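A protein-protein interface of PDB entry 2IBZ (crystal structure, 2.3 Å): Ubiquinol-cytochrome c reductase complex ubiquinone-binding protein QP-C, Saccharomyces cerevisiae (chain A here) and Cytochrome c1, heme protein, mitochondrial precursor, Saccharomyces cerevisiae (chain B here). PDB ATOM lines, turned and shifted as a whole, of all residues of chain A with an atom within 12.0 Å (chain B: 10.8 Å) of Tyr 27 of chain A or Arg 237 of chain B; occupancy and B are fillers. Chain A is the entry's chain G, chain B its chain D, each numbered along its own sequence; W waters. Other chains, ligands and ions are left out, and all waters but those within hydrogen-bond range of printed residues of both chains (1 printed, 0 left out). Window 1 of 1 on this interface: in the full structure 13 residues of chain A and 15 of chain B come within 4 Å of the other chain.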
ATOM      1  N   TRP A  13      16.055  14.637  19.207  1.00  0.00           N
ATOM      2  CA  TRP A  13      15.942  13.179  19.313  1.00  0.00           C
ATOM      3  C   TRP A  13      14.628  12.735  19.945  1.00  0.00           C
ATOM      4  O   TRP A  13      14.317  13.110  21.088  1.00  0.00           O
ATOM      5  CB  TRP A  13      17.115  12.632  20.116  1.00  0.00           C
ATOM      6  CG  TRP A  13      18.421  13.003  19.511  1.00  0.00           C
ATOM      7  CD1 TRP A  13      19.317  13.900  19.993  1.00  0.00           C
ATOM      8  CD2 TRP A  13      18.984  12.476  18.304  1.00  0.00           C
ATOM      9  NE1 TRP A  13      20.411  13.968  19.164  1.00  0.00           N
ATOM     10  CE2 TRP A  13      20.236  13.100  18.122  1.00  0.00           C
ATOM     11  CE3 TRP A  13      18.552  11.528  17.361  1.00  0.00           C
ATOM     12  CZ2 TRP A  13      21.078  12.806  17.030  1.00  0.00           C
ATOM     13  CZ3 TRP A  13      19.387  11.230  16.273  1.00  0.00           C
ATOM     14  CH2 TRP A  13      20.637  11.867  16.120  1.00  0.00           C
ATOM     15  N   MET A  16      12.026  14.689  16.020  1.00  0.00           N
ATOM     16  CA  MET A  16      12.757  15.422  14.994  1.00  0.00           C
ATOM     17  C   MET A  16      11.898  16.258  14.069  1.00  0.00           C
ATOM     18  O   MET A  16      12.372  17.256  13.518  1.00  0.00           O
ATOM     19  CB  MET A  16      13.636  14.483  14.173  1.00  0.00           C
ATOM     20  CG  MET A  16      14.905  15.143  13.651  1.00  0.00           C
ATOM     21  SD  MET A  16      16.023  15.628  14.987  1.00  0.00           S
ATOM     22  CE  MET A  16      16.731  14.035  15.419  1.00  0.00           C
ATOM     23  N   GLN A  21       7.746   7.027  10.474  1.00  0.00           N
ATOM     24  CA  GLN A  21       8.413   5.980   9.706  1.00  0.00           C
ATOM     25  C   GLN A  21       7.905   4.605  10.100  1.00  0.00           C
ATOM     26  O   GLN A  21       7.712   4.328  11.277  1.00  0.00           O
ATOM     27  CB  GLN A  21       9.935   6.050   9.910  1.00  0.00           C
ATOM     28  CG  GLN A  21      10.590   7.329   9.399  1.00  0.00           C
ATOM     29  CD  GLN A  21      12.096   7.331   9.605  1.00  0.00           C
ATOM     30  OE1 GLN A  21      12.717   6.274   9.666  1.00  0.00           O
ATOM     31  NE2 GLN A  21      12.690   8.518   9.718  1.00  0.00           N
ATOM     32  N   GLY A  23       8.053   0.317   8.346  1.00  0.00           N
ATOM     33  CA  GLY A  23       8.454  -0.544   7.253  1.00  0.00           C
ATOM     34  C   GLY A  23       9.921  -0.551   6.872  1.00  0.00           C
ATOM     35  O   GLY A  23      10.368  -1.442   6.146  1.00  0.00           O
ATOM     36  N   ILE A  24      10.666   0.460   7.308  1.00  0.00           N
ATOM     37  CA  ILE A  24      12.095   0.546   7.001  1.00  0.00           C
ATOM     38  C   ILE A  24      12.875  -0.122   8.135  1.00  0.00           C
ATOM     39  O   ILE A  24      12.649   0.176   9.304  1.00  0.00           O
ATOM     40  CB  ILE A  24      12.541   2.021   6.887  1.00  0.00           C
ATOM     41  CG1 ILE A  24      11.676   2.748   5.852  1.00  0.00           C
ATOM     42  CG2 ILE A  24      14.034   2.103   6.556  1.00  0.00           C
ATOM     43  CD1 ILE A  24      11.707   4.258   5.955  1.00  0.00           C
ATOM     44  N   THR A  25      13.785  -1.020   7.781  1.00  0.00           N
ATOM     45  CA  THR A  25      14.602  -1.733   8.751  1.00  0.00           C
ATOM     46  C   THR A  25      16.060  -1.508   8.374  1.00  0.00           C
ATOM     47  O   THR A  25      16.437  -1.728   7.221  1.00  0.00           O
ATOM     48  CB  THR A  25      14.282  -3.261   8.707  1.00  0.00           C
ATOM     49  OG1 THR A  25      12.919  -3.461   9.088  1.00  0.00           O
ATOM     50  CG2 THR A  25      15.187  -4.062   9.634  1.00  0.00           C
ATOM     51  N   SER A  26      16.885  -1.070   9.326  1.00  0.00           N
ATOM     52  CA  SER A  26      18.290  -0.829   9.014  1.00  0.00           C
ATOM     53  C   SER A  26      19.203  -1.811   9.704  1.00  0.00           C
ATOM     54  O   SER A  26      18.862  -2.368  10.736  1.00  0.00           O
ATOM     55  CB  SER A  26      18.699   0.613   9.348  1.00  0.00           C
ATOM     56  OG  SER A  26      18.643   0.867  10.739  1.00  0.00           O
ATOM     57  N   TYR A  27      20.373  -2.021   9.128  1.00  0.00           N
ATOM     58  CA  TYR A  27      21.335  -2.951   9.696  1.00  0.00           C
ATOM     59  C   TYR A  27      22.706  -2.319   9.632  1.00  0.00           C
ATOM     60  O   TYR A  27      23.004  -1.590   8.686  1.00  0.00           O
ATOM     61  CB  TYR A  27      21.384  -4.250   8.878  1.00  0.00           C
ATOM     62  CG  TYR A  27      20.073  -4.993   8.741  1.00  0.00           C
ATOM     63  CD1 TYR A  27      19.134  -4.621   7.776  1.00  0.00           C
ATOM     64  CD2 TYR A  27      19.799  -6.111   9.531  1.00  0.00           C
ATOM     65  CE1 TYR A  27      17.962  -5.345   7.601  1.00  0.00           C
ATOM     66  CE2 TYR A  27      18.631  -6.849   9.357  1.00  0.00           C
ATOM     67  CZ  TYR A  27      17.719  -6.465   8.392  1.00  0.00           C
ATOM     68  OH  TYR A  27      16.572  -7.209   8.200  1.00  0.00           O
ATOM     69  N   ALA A  28      23.554  -2.636  10.605  1.00  0.00           N
ATOM     70  CA  ALA A  28      24.910  -2.112  10.623  1.00  0.00           C
ATOM     71  C   ALA A  28      25.819  -3.077  11.386  1.00  0.00           C
ATOM     72  O   ALA A  28      25.348  -3.901  12.168  1.00  0.00           O
ATOM     73  CB  ALA A  28      24.945  -0.700  11.255  1.00  0.00           C
ATOM     74  N   VAL A  29      27.124  -2.916  11.202  1.00  0.00           N
ATOM     75  CA  VAL A  29      28.105  -3.773  11.836  1.00  0.00           C
ATOM     76  C   VAL A  29      29.207  -2.927  12.465  1.00  0.00           C
ATOM     77  O   VAL A  29      29.711  -1.985  11.846  1.00  0.00           O
ATOM     78  CB  VAL A  29      28.731  -4.751  10.790  1.00  0.00           C
ATOM     79  CG1 VAL A  29      29.953  -5.447  11.370  1.00  0.00           C
ATOM     80  CG2 VAL A  29      27.701  -5.799  10.374  1.00  0.00           C
ATOM     81  N   SER A  30      29.595  -3.291  13.681  1.00  0.00           N
ATOM     82  CA  SER A  30      30.627  -2.576  14.404  1.00  0.00           C
ATOM     83  C   SER A  30      31.890  -2.356  13.589  1.00  0.00           C
ATOM     84  O   SER A  30      32.336  -3.246  12.855  1.00  0.00           O
ATOM     85  CB  SER A  30      30.997  -3.320  15.689  1.00  0.00           C
ATOM     86  OG  SER A  30      32.142  -2.745  16.307  1.00  0.00           O
ATOM     87  N   PRO A  31      32.438  -1.131  13.653  1.00  0.00           N
ATOM     88  CA  PRO A  31      33.662  -0.766  12.942  1.00  0.00           C
ATOM     89  C   PRO A  31      34.782  -1.660  13.448  1.00  0.00           C
ATOM     90  O   PRO A  31      35.750  -1.905  12.743  1.00  0.00           O
ATOM     91  CB  PRO A  31      33.882   0.679  13.382  1.00  0.00           C
ATOM     92  CG  PRO A  31      32.477   1.192  13.474  1.00  0.00           C
ATOM     93  CD  PRO A  31      31.780   0.069  14.208  1.00  0.00           C
ATOM     94  N   ALA A  33      34.592  -4.856  14.110  1.00  0.00           N
ATOM     95  CA  ALA A  33      34.497  -6.123  13.399  1.00  0.00           C
ATOM     96  C   ALA A  33      34.823  -6.008  11.912  1.00  0.00           C
ATOM     97  O   ALA A  33      34.843  -7.012  11.201  1.00  0.00           O
ATOM     98  CB  ALA A  33      33.093  -6.697  13.569  1.00  0.00           C
ATOM     99  N   GLN A  34      35.063  -4.790  11.438  1.00  0.00           N
ATOM    100  CA  GLN A  34      35.348  -4.580  10.029  1.00  0.00           C
ATOM    101  C   GLN A  34      36.820  -4.617   9.684  1.00  0.00           C
ATOM    102  O   GLN A  34      37.688  -4.360  10.520  1.00  0.00           O
ATOM    103  CB  GLN A  34      34.714  -3.280   9.534  1.00  0.00           C
ATOM    104  CG  GLN A  34      33.203  -3.242   9.703  1.00  0.00           C
ATOM    105  CD  GLN A  34      32.569  -1.994   9.115  1.00  0.00           C
ATOM    106  OE1 GLN A  34      33.056  -1.444   8.128  1.00  0.00           O
ATOM    107  NE2 GLN A  34      31.466  -1.553   9.709  1.00  0.00           N
ATOM    108  N   LYS B 228      37.792   7.493   9.184  1.00  0.00           N
ATOM    109  CA  LYS B 228      37.231   6.366   8.450  1.00  0.00           C
ATOM    110  C   LYS B 228      36.782   5.265   9.408  1.00  0.00           C
ATOM    111  O   LYS B 228      35.716   4.680   9.230  1.00  0.00           O
ATOM    112  CB  LYS B 228      38.242   5.815   7.447  1.00  0.00           C
ATOM    113  CG  LYS B 228      38.515   6.726   6.254  1.00  0.00           C
ATOM    114  CD  LYS B 228      39.596   6.130   5.342  1.00  0.00           C
ATOM    115  CE  LYS B 228      39.749   6.916   4.039  1.00  0.00           C
ATOM    116  NZ  LYS B 228      38.499   6.923   3.201  1.00  0.00           N
ATOM    117  N   LYS B 230      35.913   5.628  12.646  1.00  0.00           N
ATOM    118  CA  LYS B 230      34.737   6.095  13.369  1.00  0.00           C
ATOM    119  C   LYS B 230      33.460   6.149  12.537  1.00  0.00           C
ATOM    120  O   LYS B 230      32.355   6.086  13.086  1.00  0.00           O
ATOM    121  CB  LYS B 230      35.019   7.434  14.054  1.00  0.00           C
ATOM    122  CG  LYS B 230      35.916   7.271  15.262  1.00  0.00           C
ATOM    123  CD  LYS B 230      36.137   8.564  16.010  1.00  0.00           C
ATOM    124  CE  LYS B 230      37.050   8.346  17.228  1.00  0.00           C
ATOM    125  NZ  LYS B 230      36.642   7.148  18.048  1.00  0.00           N
ATOM    126  N   TRP B 231      33.618   6.205  11.216  1.00  0.00           N
ATOM    127  CA  TRP B 231      32.482   6.253  10.297  1.00  0.00           C
ATOM    128  C   TRP B 231      32.099   4.909   9.625  1.00  0.00           C
ATOM    129  O   TRP B 231      31.038   4.828   8.977  1.00  0.00           O
ATOM    130  CB  TRP B 231      32.744   7.292   9.190  1.00  0.00           C
ATOM    131  CG  TRP B 231      32.426   8.697   9.563  1.00  0.00           C
ATOM    132  CD1 TRP B 231      33.148   9.512  10.386  1.00  0.00           C
ATOM    133  CD2 TRP B 231      31.289   9.461   9.139  1.00  0.00           C
ATOM    134  NE1 TRP B 231      32.530  10.733  10.505  1.00  0.00           N
ATOM    135  CE2 TRP B 231      31.385  10.728   9.754  1.00  0.00           C
ATOM    136  CE3 TRP B 231      30.191   9.192   8.306  1.00  0.00           C
ATOM    137  CZ2 TRP B 231      30.418  11.731   9.569  1.00  0.00           C
ATOM    138  CZ3 TRP B 231      29.229  10.191   8.124  1.00  0.00           C
ATOM    139  CH2 TRP B 231      29.352  11.445   8.756  1.00  0.00           C
ATOM    140  N   ALA B 232      32.929   3.868   9.788  1.00  0.00           N
ATOM    141  CA  ALA B 232      32.675   2.566   9.136  1.00  0.00           C
ATOM    142  C   ALA B 232      31.275   1.984   9.332  1.00  0.00           C
ATOM    143  O   ALA B 232      30.687   1.451   8.394  1.00  0.00           O
ATOM    144  CB  ALA B 232      33.755   1.532   9.502  1.00  0.00           C
ATOM    145  N   GLY B 233      30.724   2.113  10.529  1.00  0.00           N
ATOM    146  CA  GLY B 233      29.388   1.606  10.753  1.00  0.00           C
ATOM    147  C   GLY B 233      28.332   2.333   9.933  1.00  0.00           C
ATOM    148  O   GLY B 233      27.388   1.711   9.442  1.00  0.00           O
ATOM    149  N   ILE B 234      28.493   3.647   9.773  1.00  0.00           N
ATOM    150  CA  ILE B 234      27.533   4.474   9.024  1.00  0.00           C
ATOM    151  C   ILE B 234      27.670   4.284   7.511  1.00  0.00           C
ATOM    152  O   ILE B 234      26.682   4.116   6.799  1.00  0.00           O
ATOM    153  CB  ILE B 234      27.685   5.998   9.410  1.00  0.00           C
ATOM    154  CG1 ILE B 234      27.253   6.211  10.862  1.00  0.00           C
ATOM    155  CG2 ILE B 234      26.873   6.905   8.483  1.00  0.00           C
ATOM    156  CD1 ILE B 234      25.812   5.848  11.143  1.00  0.00           C
ATOM    157  N   LYS B 235      28.907   4.253   7.038  1.00  0.00           N
ATOM    158  CA  LYS B 235      29.173   4.092   5.623  1.00  0.00           C
ATOM    159  C   LYS B 235      28.692   2.766   5.048  1.00  0.00           C
ATOM    160  O   LYS B 235      28.195   2.722   3.924  1.00  0.00           O
ATOM    161  CB  LYS B 235      30.662   4.253   5.354  1.00  0.00           C
ATOM    162  CG  LYS B 235      31.187   5.653   5.562  1.00  0.00           C
ATOM    163  CD  LYS B 235      31.004   6.502   4.318  1.00  0.00           C
ATOM    164  CE  LYS B 235      31.660   7.862   4.494  1.00  0.00           C
ATOM    165  NZ  LYS B 235      31.665   8.683   3.260  1.00  0.00           N
ATOM    166  N   THR B 236      28.842   1.687   5.805  1.00  0.00           N
ATOM    167  CA  THR B 236      28.428   0.379   5.312  1.00  0.00           C
ATOM    168  C   THR B 236      27.030  -0.033   5.742  1.00  0.00           C
ATOM    169  O   THR B 236      26.582  -1.126   5.446  1.00  0.00           O
ATOM    170  CB  THR B 236      29.452  -0.703   5.690  1.00  0.00           C
ATOM    171  OG1 THR B 236      29.643  -0.702   7.110  1.00  0.00           O
ATOM    172  CG2 THR B 236      30.787  -0.423   4.989  1.00  0.00           C
ATOM    173  N   ARG B 237      26.338   0.871   6.417  1.00  0.00           N
ATOM    174  CA  ARG B 237      24.980   0.651   6.896  1.00  0.00           C
ATOM    175  C   ARG B 237      24.089   0.269   5.706  1.00  0.00           C
ATOM    176  O   ARG B 237      24.301   0.758   4.596  1.00  0.00           O
ATOM    177  CB  ARG B 237      24.504   1.958   7.543  1.00  0.00           C
ATOM    178  CG  ARG B 237      23.142   1.959   8.184  1.00  0.00           C
ATOM    179  CD  ARG B 237      22.961   3.261   8.977  1.00  0.00           C
ATOM    180  NE  ARG B 237      23.198   4.452   8.160  1.00  0.00           N
ATOM    181  CZ  ARG B 237      22.614   5.634   8.362  1.00  0.00           C
ATOM    182  NH1 ARG B 237      22.882   6.651   7.552  1.00  0.00           N
ATOM    183  NH2 ARG B 237      21.784   5.810   9.385  1.00  0.00           N
ATOM    184  N   LYS B 238      23.128  -0.630   5.929  1.00  0.00           N
ATOM    185  CA  LYS B 238      22.217  -1.069   4.867  1.00  0.00           C
ATOM    186  C   LYS B 238      20.755  -0.992   5.267  1.00  0.00           C
ATOM    187  O   LYS B 238      20.390  -1.321   6.394  1.00  0.00           O
ATOM    188  CB  LYS B 238      22.554  -2.493   4.418  1.00  0.00           C
ATOM    189  CG  LYS B 238      23.977  -2.625   3.919  1.00  0.00           C
ATOM    190  CD  LYS B 238      24.190  -3.831   3.040  1.00  0.00           C
ATOM    191  CE  LYS B 238      25.615  -3.835   2.501  1.00  0.00           C
ATOM    192  NZ  LYS B 238      25.850  -4.932   1.505  1.00  0.00           N
ATOM    193  N   PHE B 239      19.918  -0.558   4.332  1.00  0.00           N
ATOM    194  CA  PHE B 239      18.481  -0.427   4.575  1.00  0.00           C
ATOM    195  C   PHE B 239      17.626  -1.406   3.731  1.00  0.00           C
ATOM    196  O   PHE B 239      18.051  -1.873   2.663  1.00  0.00           O
ATOM    197  CB  PHE B 239      18.022   1.012   4.272  1.00  0.00           C
ATOM    198  CG  PHE B 239      18.542   2.046   5.235  1.00  0.00           C
ATOM    199  CD1 PHE B 239      19.810   2.604   5.068  1.00  0.00           C
ATOM    200  CD2 PHE B 239      17.763   2.470   6.309  1.00  0.00           C
ATOM    201  CE1 PHE B 239      20.299   3.569   5.960  1.00  0.00           C
ATOM    202  CE2 PHE B 239      18.240   3.432   7.208  1.00  0.00           C
ATOM    203  CZ  PHE B 239      19.513   3.981   7.029  1.00  0.00           C
ATOM    204  N   VAL B 240      16.441  -1.740   4.247  1.00  0.00           N
ATOM    205  CA  VAL B 240      15.483  -2.598   3.548  1.00  0.00           C
ATOM    206  C   VAL B 240      14.072  -2.073   3.807  1.00  0.00           C
ATOM    207  O   VAL B 240      13.716  -1.730   4.927  1.00  0.00           O
ATOM    208  CB  VAL B 240      15.545  -4.084   3.977  1.00  0.00           C
ATOM    209  CG1 VAL B 240      16.866  -4.692   3.594  1.00  0.00           C
ATOM    210  CG2 VAL B 240      15.291  -4.226   5.462  1.00  0.00           C
ATOM    211  N   PHE B 241      13.270  -2.004   2.759  1.00  0.00           N
ATOM    212  CA  PHE B 241      11.908  -1.518   2.898  1.00  0.00           C
ATOM    213  C   PHE B 241      10.890  -2.631   2.602  1.00  0.00           C
ATOM    214  O   PHE B 241      11.016  -3.363   1.618  1.00  0.00           O
ATOM    215  CB  PHE B 241      11.707  -0.338   1.948  1.00  0.00           C
ATOM    216  CG  PHE B 241      10.339   0.284   2.008  1.00  0.00           C
ATOM    217  CD1 PHE B 241       9.773   0.669   3.229  1.00  0.00           C
ATOM    218  CD2 PHE B 241       9.633   0.539   0.837  1.00  0.00           C
ATOM    219  CE1 PHE B 241       8.527   1.302   3.284  1.00  0.00           C
ATOM    220  CE2 PHE B 241       8.384   1.171   0.879  1.00  0.00           C
ATOM    221  CZ  PHE B 241       7.831   1.555   2.109  1.00  0.00           C
ATOM    222  N   ASN B 242       9.939  -2.796   3.512  1.00  0.00           N
ATOM    223  CA  ASN B 242       8.863  -3.763   3.367  1.00  0.00           C
ATOM    224  C   ASN B 242       7.605  -2.932   3.597  1.00  0.00           C
ATOM    225  O   ASN B 242       7.228  -2.673   4.738  1.00  0.00           O
ATOM    226  CB  ASN B 242       8.969  -4.880   4.414  1.00  0.00           C
ATOM    227  CG  ASN B 242      10.083  -5.855   4.112  1.00  0.00           C
ATOM    228  OD1 ASN B 242      10.265  -6.267   2.972  1.00  0.00           O
ATOM    229  ND2 ASN B 242      10.834  -6.236   5.132  1.00  0.00           N
HETATM  230  O   HOH W   1      27.485  -1.119   9.110  1.00  0.00           O
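Of the 14 printed residues of chain B, 9 touch a printed residue of chain A. Hydrophobic or aromatic side chains of chain B that line the printed part of chain A: Ala 232, Phe 239, Val 240 and Phe 241. Hydrophobic or aromatic side chains of chain A that line the printed part of chain B: Ile 24, Tyr 27, Ala 28 and Pro 31. Among the printed residues, 20 pairs touch across the chains. Among the printed residues, no Asp or Glu carboxylate lies within 4 Å of a Lys or Arg side-chain nitrogen of the other chain.
The backbone carbonyl oxygen of Lys 238 of chain B is in hydrogen-bond range of the backbone NH of Tyr 27 of chain A (2.8 Å). The backbone NH (N) of Asn 242 of chain B lies within hydrogen-bond range of the backbone carbonyl oxygen (O) of Gly 23 of chain A (3.0 Å). The backbone NH (N) of Thr 25 of chain A is in hydrogen-bond range of the backbone carbonyl oxygen (O) of Val 240 of chain B. The backbone carbonyl oxygen of Ala 232 of chain B lies within hydrogen-bond range of the side-chain amide nitrogen of Gln 34 of chain A (3.4 Å). The side-chain hydroxyl of Thr 236 of chain B is in hydrogen-bond range of the side-chain amide nitrogen of Gln 34 of chain A, 3.3 Å away.
Of the printed residues of chain B, Tyr 27 of chain A touches Arg 237 (3.5 Å), Lys 238 (2.8 Å) and Val 240 (3.6 Å). Of chain A, only Tyr 27 (3.5 Å) comes within 4 Å of Arg 237 of chain B. Thr 25 of chain A touches just these residues of chain B: Phe 239 (3.6 Å) and Val 240 (2.9 Å). Ala 28 of chain A touches just one residue of chain B: Gly 233. Of chain A, only Ala 28 (3.9 Å), Val 29 (3.8 Å), Pro 31 (3.5 Å) and Gln 34 (3.8 Å) come within 4 Å of Gly 233 of chain B. Of chain A, only Gln 34 (3.3 Å) comes within 4 Å of Thr 236 of chain B. Of chain A, only Ser 26 and Tyr 27 come within 4 Å of Lys 238 of chain B. Of chain A, only Gly 23 (3.6 Å), Ile 24 (3.5 Å), Thr 25 (2.9 Å) and Tyr 27 (3.6 Å) come within 4 Å of Val 240 of chain B. Printed residues of chain B within 4 Å of Ile 24 of chain A: Phe 239, Val 240 and Phe 241. Of the printed residues of chain B, Gly 23 of chain A touches Val 240, Phe 241 and Asn 242. Of the printed residues of chain B, Pro 31 of chain A touches Ala 232 and Gly 233. Of the printed residues of chain A, Ala 232 of chain B touches Pro 31 and Gln 34. Printed residues of chain A within 4 Å of Asn 242 of chain B: Gly 23 (3.0 Å). Lys 230 of chain B touches none of the printed residues of chain A. Ser 30 of chain A touches none of the printed residues of chain B.
The backbone carbonyl oxygen of Ala 232 of chain B sits at hydrogen-bond distance from the side-chain hydroxyl of Thr 236 of chain B (2.7 Å). O of Val 29 of chain A lies within hydrogen-bond range of NE2 of Gln 34 of chain A, at 2.8 Å.
Gly 23 of chain A touches Val 240 of chain B (O to O, 3.6 Å). Gly 23 of chain A touches Phe 241 of chain B (O to CA, 3.6 Å). O of Val 240 of chain B touches CA of Ile 24 of chain A, at 3.5 Å. Ser 26 of chain A touches Lys 238 of chain B. CE2 of Phe 239 of chain B touches CB of Ser 26 of chain A, 3.6 Å away. Val 240 of chain B touches Tyr 27 of chain A (CG2 to CE1, 3.6 Å). Val 29 of chain A touches Gly 233 of chain B. Pro 31 of chain A touches Ala 232 of chain B. Gly 233 of chain B touches Pro 31 of chain A (N to CG, 3.5 Å). Gln 34 of chain A touches Gly 233 of chain B.
Water W1 lies within hydrogen-bond range of the backbone NH (N) of Val 29 of chain A, the backbone carbonyl oxygen (O) of Gly 233 of chain B and the side-chain hydroxyl (OG1) of Thr 236 of chain B.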
